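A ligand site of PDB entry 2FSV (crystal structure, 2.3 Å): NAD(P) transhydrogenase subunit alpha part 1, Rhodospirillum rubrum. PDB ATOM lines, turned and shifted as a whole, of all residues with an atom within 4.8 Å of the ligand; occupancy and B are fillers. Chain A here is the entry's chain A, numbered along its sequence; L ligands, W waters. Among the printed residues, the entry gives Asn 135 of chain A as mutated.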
ATOM      1  N   ARG A 127     -15.679   9.907  -4.187  1.00  0.00           N
ATOM      2  CA  ARG A 127     -15.470  11.301  -4.567  1.00  0.00           C
ATOM      3  C   ARG A 127     -16.515  12.235  -3.966  1.00  0.00           C
ATOM      4  O   ARG A 127     -17.334  12.826  -4.688  1.00  0.00           O
ATOM      5  CB  ARG A 127     -15.438  11.445  -6.093  1.00  0.00           C
ATOM      6  CG  ARG A 127     -14.156  10.955  -6.736  1.00  0.00           C
ATOM      7  CD  ARG A 127     -14.127  11.366  -8.186  1.00  0.00           C
ATOM      8  NE  ARG A 127     -12.798  11.247  -8.777  1.00  0.00           N
ATOM      9  CZ  ARG A 127     -12.414  11.858  -9.899  1.00  0.00           C
ATOM     10  NH1 ARG A 127     -13.253  12.636 -10.587  1.00  0.00           N
ATOM     11  NH2 ARG A 127     -11.181  11.684 -10.357  1.00  0.00           N
ATOM     12  N   GLN A 132     -12.076  14.518   0.860  1.00  0.00           N
ATOM     13  CA  GLN A 132     -10.901  15.154   0.226  1.00  0.00           C
ATOM     14  C   GLN A 132      -9.673  15.129   1.125  1.00  0.00           C
ATOM     15  O   GLN A 132      -8.542  15.044   0.636  1.00  0.00           O
ATOM     16  CB  GLN A 132     -11.211  16.591  -0.185  1.00  0.00           C
ATOM     17  CG  GLN A 132     -11.834  16.727  -1.564  1.00  0.00           C
ATOM     18  CD  GLN A 132     -10.812  16.563  -2.682  1.00  0.00           C
ATOM     19  OE1 GLN A 132     -10.674  15.483  -3.260  1.00  0.00           O
ATOM     20  NE2 GLN A 132     -10.079  17.632  -2.981  1.00  0.00           N
ATOM     21  N   ASN A 135      -8.095  11.661   0.658  1.00  0.00           N
ATOM     22  CA  ASN A 135      -7.919  11.289  -0.753  1.00  0.00           C
ATOM     23  C   ASN A 135      -6.431  11.195  -1.118  1.00  0.00           C
ATOM     24  O   ASN A 135      -5.769  12.221  -1.310  1.00  0.00           O
ATOM     25  CB  ASN A 135      -8.620  12.318  -1.642  1.00  0.00           C
ATOM     26  CG  ASN A 135      -8.658  11.906  -3.121  1.00  0.00           C
ATOM     27  OD1 ASN A 135      -7.947  11.009  -3.564  1.00  0.00           O
ATOM     28  ND2 ASN A 135      -9.493  12.580  -3.883  1.00  0.00           N
ATOM     29  N   LEU A 137      -5.148   9.967  -3.925  1.00  0.00           N
ATOM     30  CA  LEU A 137      -4.921  10.233  -5.341  1.00  0.00           C
ATOM     31  C   LEU A 137      -4.637  11.716  -5.616  1.00  0.00           C
ATOM     32  O   LEU A 137      -3.679  12.035  -6.323  1.00  0.00           O
ATOM     33  CB  LEU A 137      -6.098   9.743  -6.200  1.00  0.00           C
ATOM     34  CG  LEU A 137      -6.330   8.228  -6.261  1.00  0.00           C
ATOM     35  CD1 LEU A 137      -7.536   7.901  -7.131  1.00  0.00           C
ATOM     36  CD2 LEU A 137      -5.099   7.472  -6.772  1.00  0.00           C
ATOM     37  N   SER A 138      -5.457  12.594  -5.058  1.00  0.00           N
ATOM     38  CA  SER A 138      -5.274  14.039  -5.248  1.00  0.00           C
ATOM     39  C   SER A 138      -4.067  14.607  -4.493  1.00  0.00           C
ATOM     40  O   SER A 138      -3.383  15.485  -5.002  1.00  0.00           O
ATOM     41  CB  SER A 138      -6.538  14.802  -4.825  1.00  0.00           C
ATOM     42  OG  SER A 138      -6.815  14.601  -3.459  1.00  0.00           O
ATOM     43  N   SER A 141      -0.976  13.236  -6.626  1.00  0.00           N
ATOM     44  CA  SER A 141      -0.938  13.766  -7.993  1.00  0.00           C
ATOM     45  C   SER A 141      -0.713  15.279  -8.023  1.00  0.00           C
ATOM     46  O   SER A 141      -0.187  15.795  -9.013  1.00  0.00           O
ATOM     47  CB  SER A 141      -2.222  13.425  -8.743  1.00  0.00           C
ATOM     48  OG  SER A 141      -3.326  14.096  -8.174  1.00  0.00           O
ATOM     49  N   GLY A 179      -4.651  17.997 -20.091  1.00  0.00           N
ATOM     50  CA  GLY A 179      -5.391  17.447 -18.955  1.00  0.00           C
ATOM     51  C   GLY A 179      -5.174  18.320 -17.726  1.00  0.00           C
ATOM     52  O   GLY A 179      -4.068  18.383 -17.194  1.00  0.00           O
ATOM     53  N   VAL A 180      -6.244  18.981 -17.283  1.00  0.00           N
ATOM     54  CA  VAL A 180      -6.185  19.915 -16.158  1.00  0.00           C
ATOM     55  C   VAL A 180      -7.030  19.379 -15.002  1.00  0.00           C
ATOM     56  O   VAL A 180      -8.021  19.989 -14.589  1.00  0.00           O
ATOM     57  CB  VAL A 180      -6.622  21.322 -16.594  1.00  0.00           C
ATOM     58  CG1 VAL A 180      -6.365  22.365 -15.490  1.00  0.00           C
ATOM     59  CG2 VAL A 180      -5.877  21.758 -17.863  1.00  0.00           C
ATOM     60  N   GLY A 181      -6.614  18.226 -14.487  1.00  0.00           N
ATOM     61  CA  GLY A 181      -7.112  17.726 -13.208  1.00  0.00           C
ATOM     62  C   GLY A 181      -6.240  18.279 -12.096  1.00  0.00           C
ATOM     63  O   GLY A 181      -5.744  19.405 -12.207  1.00  0.00           O
ATOM     64  N   VAL A 182      -6.030  17.491 -11.049  1.00  0.00           N
ATOM     65  CA  VAL A 182      -5.237  17.938  -9.894  1.00  0.00           C
ATOM     66  C   VAL A 182      -3.771  18.139 -10.273  1.00  0.00           C
ATOM     67  O   VAL A 182      -3.165  19.165  -9.921  1.00  0.00           O
ATOM     68  CB  VAL A 182      -5.336  16.955  -8.699  1.00  0.00           C
ATOM     69  CG1 VAL A 182      -4.517  17.463  -7.502  1.00  0.00           C
ATOM     70  CG2 VAL A 182      -6.794  16.745  -8.258  1.00  0.00           C
ATOM     71  N   ALA A 183      -3.197  17.175 -10.983  1.00  0.00           N
ATOM     72  CA  ALA A 183      -1.794  17.265 -11.432  1.00  0.00           C
ATOM     73  C   ALA A 183      -1.586  18.411 -12.415  1.00  0.00           C
ATOM     74  O   ALA A 183      -0.617  19.156 -12.308  1.00  0.00           O
ATOM     75  CB  ALA A 183      -1.343  15.940 -12.039  1.00  0.00           C
ATOM     76  N   LEU A 185      -3.350  21.231 -12.818  1.00  0.00           N
ATOM     77  CA  LEU A 185      -3.457  22.542 -12.180  1.00  0.00           C
ATOM     78  C   LEU A 185      -2.130  22.977 -11.526  1.00  0.00           C
ATOM     79  O   LEU A 185      -1.715  24.135 -11.650  1.00  0.00           O
ATOM     80  CB  LEU A 185      -4.581  22.564 -11.140  1.00  0.00           C
ATOM     81  CG  LEU A 185      -6.010  22.535 -11.690  1.00  0.00           C
ATOM     82  CD1 LEU A 185      -7.007  22.076 -10.609  1.00  0.00           C
ATOM     83  CD2 LEU A 185      -6.418  23.886 -12.241  1.00  0.00           C
ATOM     84  N   THR A 201      -5.201  22.555 -22.168  1.00  0.00           N
ATOM     85  CA  THR A 201      -6.427  22.046 -22.771  1.00  0.00           C
ATOM     86  C   THR A 201      -6.955  20.851 -21.982  1.00  0.00           C
ATOM     87  O   THR A 201      -6.189  20.096 -21.389  1.00  0.00           O
ATOM     88  CB  THR A 201      -6.236  21.669 -24.261  1.00  0.00           C
ATOM     89  OG1 THR A 201      -7.517  21.417 -24.865  1.00  0.00           O
ATOM     90  CG2 THR A 201      -5.337  20.440 -24.428  1.00  0.00           C
ATOM     91  N   ASP A 202      -8.275  20.705 -22.001  1.00  0.00           N
ATOM     92  CA  ASP A 202      -8.969  19.621 -21.327  1.00  0.00           C
ATOM     93  C   ASP A 202     -10.341  19.475 -21.987  1.00  0.00           C
ATOM     94  O   ASP A 202     -10.827  20.402 -22.630  1.00  0.00           O
ATOM     95  CB  ASP A 202      -9.128  19.929 -19.835  1.00  0.00           C
ATOM     96  CG  ASP A 202      -9.420  18.697 -19.001  1.00  0.00           C
ATOM     97  OD1 ASP A 202     -10.337  17.925 -19.342  1.00  0.00           O
ATOM     98  OD2 ASP A 202      -8.724  18.501 -17.981  1.00  0.00           O
ATOM     99  N   VAL A 203     -10.959  18.315 -21.802  1.00  0.00           N
ATOM    100  CA  VAL A 203     -12.294  18.044 -22.353  1.00  0.00           C
ATOM    101  C   VAL A 203     -13.434  18.573 -21.489  1.00  0.00           C
ATOM    102  O   VAL A 203     -14.540  18.795 -21.980  1.00  0.00           O
ATOM    103  CB  VAL A 203     -12.514  16.537 -22.644  1.00  0.00           C
ATOM    104  CG1 VAL A 203     -11.628  16.106 -23.804  1.00  0.00           C
ATOM    105  CG2 VAL A 203     -12.274  15.658 -21.404  1.00  0.00           C
ATOM    106  N   ARG A 204     -13.170  18.779 -20.193  1.00  0.00           N
ATOM    107  CA  ARG A 204     -14.172  19.323 -19.277  1.00  0.00           C
ATOM    108  C   ARG A 204     -14.226  20.849 -19.389  1.00  0.00           C
ATOM    109  O   ARG A 204     -13.198  21.518 -19.426  1.00  0.00           O
ATOM    110  CB  ARG A 204     -13.872  18.908 -17.838  1.00  0.00           C
ATOM    111  CG  ARG A 204     -13.910  17.401 -17.645  1.00  0.00           C
ATOM    112  CD  ARG A 204     -13.820  16.997 -16.183  1.00  0.00           C
ATOM    113  NE  ARG A 204     -12.527  17.318 -15.576  1.00  0.00           N
ATOM    114  CZ  ARG A 204     -12.280  18.363 -14.774  1.00  0.00           C
ATOM    115  NH1 ARG A 204     -13.243  19.216 -14.418  1.00  0.00           N
ATOM    116  NH2 ARG A 204     -11.055  18.548 -14.296  1.00  0.00           N
ATOM    117  N   GLY A 234     -15.957  16.250 -12.225  1.00  0.00           N
ATOM    118  CA  GLY A 234     -15.514  14.869 -12.066  1.00  0.00           C
ATOM    119  C   GLY A 234     -14.473  14.465 -13.100  1.00  0.00           C
ATOM    120  O   GLY A 234     -13.505  15.197 -13.334  1.00  0.00           O
ATOM    121  N   TYR A 235     -14.676  13.301 -13.712  1.00  0.00           N
ATOM    122  CA  TYR A 235     -13.742  12.743 -14.719  1.00  0.00           C
ATOM    123  C   TYR A 235     -14.338  12.771 -16.126  1.00  0.00           C
ATOM    124  O   TYR A 235     -15.479  13.202 -16.316  1.00  0.00           O
ATOM    125  CB  TYR A 235     -13.246  11.323 -14.340  1.00  0.00           C
ATOM    126  CG  TYR A 235     -14.155  10.485 -13.472  1.00  0.00           C
ATOM    127  CD1 TYR A 235     -15.491  10.267 -13.807  1.00  0.00           C
ATOM    128  CD2 TYR A 235     -13.671   9.892 -12.308  1.00  0.00           C
ATOM    129  CE1 TYR A 235     -16.319   9.499 -13.010  1.00  0.00           C
ATOM    130  CE2 TYR A 235     -14.491   9.123 -11.499  1.00  0.00           C
ATOM    131  CZ  TYR A 235     -15.812   8.935 -11.852  1.00  0.00           C
ATOM    132  OH  TYR A 235     -16.626   8.162 -11.056  1.00  0.00           O
ATOM    133  N   ALA A 236     -13.562  12.303 -17.101  1.00  0.00           N
ATOM    134  CA  ALA A 236     -13.920  12.368 -18.516  1.00  0.00           C
ATOM    135  C   ALA A 236     -14.399  11.012 -19.055  1.00  0.00           C
ATOM    136  O   ALA A 236     -14.366  10.003 -18.353  1.00  0.00           O
ATOM    137  CB  ALA A 236     -12.717  12.847 -19.326  1.00  0.00           C
ATOM    138  N   MET A 239     -13.591  10.041 -25.829  1.00  0.00           N
ATOM    139  CA  MET A 239     -14.136  11.010 -26.791  1.00  0.00           C
ATOM    140  C   MET A 239     -14.311  10.459 -28.205  1.00  0.00           C
ATOM    141  O   MET A 239     -15.194  10.927 -28.938  1.00  0.00           O
ATOM    142  CB  MET A 239     -13.234  12.262 -26.841  1.00  0.00           C
ATOM    143  CG  MET A 239     -13.156  13.044 -25.544  1.00  0.00           C
ATOM    144  SD  MET A 239     -14.739  13.675 -24.932  1.00  0.00           S
ATOM    145  CE  MET A 239     -15.187  14.845 -26.212  1.00  0.00           C
ATOM    146  N   GLN A 247      -9.116  17.883 -31.795  1.00  0.00           N
ATOM    147  CA  GLN A 247      -8.270  18.263 -30.670  1.00  0.00           C
ATOM    148  C   GLN A 247      -6.828  18.469 -31.126  1.00  0.00           C
ATOM    149  O   GLN A 247      -6.238  19.510 -30.857  1.00  0.00           O
ATOM    150  CB  GLN A 247      -8.310  17.194 -29.568  1.00  0.00           C
ATOM    151  CG  GLN A 247      -7.577  17.587 -28.289  1.00  0.00           C
ATOM    152  CD  GLN A 247      -7.486  16.455 -27.286  1.00  0.00           C
ATOM    153  OE1 GLN A 247      -7.680  16.671 -26.088  1.00  0.00           O
ATOM    154  NE2 GLN A 247      -7.192  15.252 -27.767  1.00  0.00           N
ATOM    155  N   THR A 264      -1.161  14.688 -18.632  1.00  0.00           N
ATOM    156  CA  THR A 264      -1.653  14.155 -17.357  1.00  0.00           C
ATOM    157  C   THR A 264      -2.990  13.407 -17.462  1.00  0.00           C
ATOM    158  O   THR A 264      -3.553  13.016 -16.436  1.00  0.00           O
ATOM    159  CB  THR A 264      -1.859  15.292 -16.321  1.00  0.00           C
ATOM    160  OG1 THR A 264      -3.097  15.973 -16.585  1.00  0.00           O
ATOM    161  CG2 THR A 264      -0.715  16.303 -16.370  1.00  0.00           C
ATOM    162  N   ALA A 265      -3.491  13.205 -18.673  1.00  0.00           N
ATOM    163  CA  ALA A 265      -4.876  12.752 -18.860  1.00  0.00           C
ATOM    164  C   ALA A 265      -5.063  11.256 -18.617  1.00  0.00           C
ATOM    165  O   ALA A 265      -4.309  10.429 -19.155  1.00  0.00           O
ATOM    166  CB  ALA A 265      -5.359  13.133 -20.252  1.00  0.00           C
ATOM    167  N   LEU A 266      -6.062  10.924 -17.797  1.00  0.00           N
ATOM    168  CA  LEU A 266      -6.497   9.542 -17.562  1.00  0.00           C
ATOM    169  C   LEU A 266      -8.003   9.398 -17.762  1.00  0.00           C
ATOM    170  O   LEU A 266      -8.751  10.372 -17.687  1.00  0.00           O
ATOM    171  CB  LEU A 266      -6.192   9.119 -16.126  1.00  0.00           C
ATOM    172  CG  LEU A 266      -4.758   9.284 -15.620  1.00  0.00           C
ATOM    173  CD1 LEU A 266      -4.717   9.013 -14.130  1.00  0.00           C
ATOM    174  CD2 LEU A 266      -3.817   8.354 -16.373  1.00  0.00           C
ATOM    175  N   ILE A 267      -8.434   8.159 -18.015  1.00  0.00           N
ATOM    176  CA  ILE A 267      -9.848   7.792 -18.095  1.00  0.00           C
ATOM    177  C   ILE A 267     -10.039   6.506 -17.280  1.00  0.00           C
ATOM    178  O   ILE A 267      -9.426   5.492 -17.597  1.00  0.00           O
ATOM    179  CB  ILE A 267     -10.294   7.551 -19.567  1.00  0.00           C
ATOM    180  CG1 ILE A 267     -10.266   8.854 -20.364  1.00  0.00           C
ATOM    181  CG2 ILE A 267     -11.721   6.970 -19.607  1.00  0.00           C
ATOM    182  CD1 ILE A 267     -10.253   8.661 -21.867  1.00  0.00           C
ATOM    183  N   PRO A 273      -5.716   8.170 -22.760  1.00  0.00           N
ATOM    184  CA  PRO A 273      -5.968   8.632 -24.127  1.00  0.00           C
ATOM    185  C   PRO A 273      -4.706   9.141 -24.806  1.00  0.00           C
ATOM    186  O   PRO A 273      -3.859   9.758 -24.156  1.00  0.00           O
ATOM    187  CB  PRO A 273      -6.954   9.785 -23.938  1.00  0.00           C
ATOM    188  CG  PRO A 273      -6.729  10.257 -22.559  1.00  0.00           C
ATOM    189  CD  PRO A 273      -6.337   9.061 -21.754  1.00  0.00           C
ATOM    190  N   LEU A 275      -2.809  11.680 -26.759  1.00  0.00           N
ATOM    191  CA  LEU A 275      -2.916  13.134 -26.922  1.00  0.00           C
ATOM    192  C   LEU A 275      -1.817  13.707 -27.805  1.00  0.00           C
ATOM    193  O   LEU A 275      -2.043  14.687 -28.514  1.00  0.00           O
ATOM    194  CB  LEU A 275      -2.892  13.810 -25.548  1.00  0.00           C
ATOM    195  CG  LEU A 275      -4.208  14.016 -24.767  1.00  0.00           C
ATOM    196  CD1 LEU A 275      -5.312  13.010 -25.070  1.00  0.00           C
ATOM    197  CD2 LEU A 275      -3.902  14.013 -23.281  1.00  0.00           C
HETATM  198  P1  LIG L   1      -7.737  12.483 -13.818  1.00  0.00           P
HETATM  199  O1  LIG L   1      -6.472  12.146 -13.069  1.00  0.00           O
HETATM  200  O2  LIG L   1      -8.795  11.409 -14.017  1.00  0.00           O
HETATM  201  O3  LIG L   1      -7.347  13.057 -15.271  1.00  0.00           O
HETATM  202  C1  LIG L   1      -6.736  14.342 -15.439  1.00  0.00           C
HETATM  203  C2  LIG L   1      -7.524  15.209 -16.425  1.00  0.00           C
HETATM  204  O4  LIG L   1      -7.475  14.622 -17.728  1.00  0.00           O
HETATM  205  C3  LIG L   1      -9.013  15.366 -16.118  1.00  0.00           C
HETATM  206  O5  LIG L   1      -9.290  16.714 -15.800  1.00  0.00           O
HETATM  207  C4  LIG L   1      -9.733  14.941 -17.390  1.00  0.00           C
HETATM  208  O6  LIG L   1     -10.866  15.720 -17.698  1.00  0.00           O
HETATM  209  C5  LIG L   1      -8.630  15.058 -18.430  1.00  0.00           C
HETATM  210  N1  LIG L   1      -8.791  14.255 -19.655  1.00  0.00           N
HETATM  211  C6  LIG L   1      -9.143  12.948 -19.757  1.00  0.00           C
HETATM  212  N2  LIG L   1      -9.183  12.522 -21.065  1.00  0.00           N
HETATM  213  C7  LIG L   1      -8.839  13.577 -21.825  1.00  0.00           C
HETATM  214  C8  LIG L   1      -8.653  13.941 -23.263  1.00  0.00           C
HETATM  215  N3  LIG L   1      -8.847  13.019 -24.236  1.00  0.00           N
HETATM  216  N4  LIG L   1      -8.277  15.206 -23.571  1.00  0.00           N
HETATM  217  C9  LIG L   1      -8.064  16.185 -22.670  1.00  0.00           C
HETATM  218  N5  LIG L   1      -8.207  15.977 -21.353  1.00  0.00           N
HETATM  219  C10 LIG L   1      -8.595  14.666 -20.901  1.00  0.00           C
HETATM  220  O7  LIG L   1      -8.464  13.747 -13.118  1.00  0.00           O
HETATM  221  P2  LIG L   1      -8.215  14.194 -11.593  1.00  0.00           P
HETATM  222  O8  LIG L   1      -6.784  14.656 -11.421  1.00  0.00           O
HETATM  223  O9  LIG L   1      -8.763  13.157 -10.650  1.00  0.00           O
HETATM  224  O10 LIG L   1      -9.148  15.478 -11.514  1.00  0.00           O
HETATM  225  C11 LIG L   1     -10.457  15.510 -12.059  1.00  0.00           C
HETATM  226  C12 LIG L   1     -11.267  16.647 -11.417  1.00  0.00           C
HETATM  227  O11 LIG L   1     -12.366  16.079 -10.687  1.00  0.00           O
HETATM  228  C13 LIG L   1     -10.458  17.539 -10.478  1.00  0.00           C
HETATM  229  O12 LIG L   1     -10.305  18.844 -11.018  1.00  0.00           O
HETATM  230  C14 LIG L   1     -11.237  17.559  -9.177  1.00  0.00           C
HETATM  231  O13 LIG L   1     -11.671  18.875  -8.864  1.00  0.00           O
HETATM  232  C15 LIG L   1     -12.433  16.624  -9.373  1.00  0.00           C
HETATM  233  N6  LIG L   1     -12.269  15.639  -8.315  1.00  0.00           N
HETATM  234  C16 LIG L   1     -11.123  14.694  -8.378  1.00  0.00           C
HETATM  235  C17 LIG L   1     -10.904  13.843  -7.372  1.00  0.00           C
HETATM  236  C18 LIG L   1      -9.782  12.903  -7.368  1.00  0.00           C
HETATM  237  O14 LIG L   1     -10.010  11.705  -7.484  1.00  0.00           O
HETATM  238  N7  LIG L   1      -8.541  13.350  -7.229  1.00  0.00           N
HETATM  239  C19 LIG L   1     -11.867  13.864  -6.219  1.00  0.00           C
HETATM  240  C20 LIG L   1     -13.047  14.792  -6.167  1.00  0.00           C
HETATM  241  C21 LIG L   1     -13.229  15.625  -7.190  1.00  0.00           C
HETATM  242  O   HOH W   1      -3.643  12.641 -13.789  1.00  0.00           O
HETATM  243  O   HOH W   2     -10.621  11.606 -16.029  1.00  0.00           O
HETATM  244  O   HOH W   3      -8.489  13.046 -27.055  1.00  0.00           O
HETATM  245  O   HOH W   4      -4.438  16.553 -14.471  1.00  0.00           O
HETATM  246  O   HOH W   5      -4.470  14.940 -12.273  1.00  0.00           O
HETATM  247  O   HOH W   6     -11.109  11.740 -23.054  1.00  0.00           O
HETATM  248  O   HOH W   7      -5.842  13.224  -9.002  1.00  0.00           O
HETATM  249  O   HOH W   8      -9.746  20.967 -12.633  1.00  0.00           O
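An oxygen (O5) of the ligand lies within hydrogen-bond range of the backbone NH of Gly 181 (3.3 Å). An oxygen (O8) of the ligand sits at hydrogen-bond distance from the backbone NH (N) of Val 182, at 3.0 Å. The guanidinium group of Arg 127 is in salt-bridge range of an oxygen (O9) of the ligand. OE1 of Gln 247 sits close to N4 of the ligand (3.0 Å). NH2 of Arg 204 sits at hydrogen-bond distance from O5 of the ligand (3.0 Å). An oxygen (O6) of the ligand lies within hydrogen-bond range of the side-chain carboxylate (OD1) of Asp 202 (2.8 Å).
The side-chain amide oxygen (OD1) of Asn 135 is in hydrogen-bond range of the backbone NH (N) of Leu 137, at 3.0 Å. The side-chain hydroxyl of Thr 264 lies within hydrogen-bond range of the backbone carbonyl oxygen of Gly 179. OG of Ser 141 lies within hydrogen-bond range of O of Ser 138 (3.5 Å). The side-chain carboxylate of Asp 202 lies within hydrogen-bond range of the backbone NH of Val 180. The side-chain carboxylate of Asp 202 is in hydrogen-bond range of the backbone NH of Arg 204, 3.1 Å away. The backbone NH (N) of Ser 138 lies within hydrogen-bond range of the side-chain amide oxygen (OD1) of Asn 135 (3.3 Å). The guanidinium group of Arg 204 sits at hydrogen-bond distance from the backbone carbonyl oxygen of Val 180 (3.4 Å). N of Gly 179 lies within hydrogen-bond range of O of Thr 201.
O of Gly 234 sits close to O11 of the ligand, 3.0 Å away. Residues that only touch the ligand: Gln 132 (3.6 Å), Asn 135 (3.5 Å), Ser 138 (3.4 Å), Gly 179 (3.7 Å), Val 180 (3.6 Å), Val 203 (3.5 Å), Ala 236 (3.6 Å), Thr 264 (3.6 Å), Ala 265 (3.4 Å), Leu 266 (3.3 Å), Ile 267 (3.9 Å), Pro 273 (3.7 Å) and Leu 275 (3.6 Å). Hydrophobic or aromatic side chains that line the ligand: Val 182, Val 203, Ala 236, Ala 265, Leu 266, Ile 267, Pro 273 and Leu 275. The nearest printed residue that does not touch the ligand is Ala 183 (4.4 Å).
Water W5 lies within hydrogen-bond range of O8 of the ligand (2.5 Å), N of Ala 183 (2.9 Å) and N of Val 182 (3.2 Å). Water W2 lies within hydrogen-bond range of O2 of the ligand, O of Leu 266 and N of Ala 236. Water W8 lies within hydrogen-bond range of an oxygen (O12) of the ligand (2.7 Å), the backbone carbonyl oxygen (O) of Val 180 (2.8 Å) and the guanidinium group (NH2) of Arg 204 (3.2 Å). Water W1 bridges the backbone carbonyl oxygen of Thr 264 (2.7 Å) and an oxygen (O1) of the ligand (3.0 Å). Water W7 bridges OG of Ser 141 (2.8 Å) and O8 of the ligand (3.0 Å). Water W4 lies within hydrogen-bond range of OG1 of Thr 264, N of Gly 181 and O of Gly 179.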
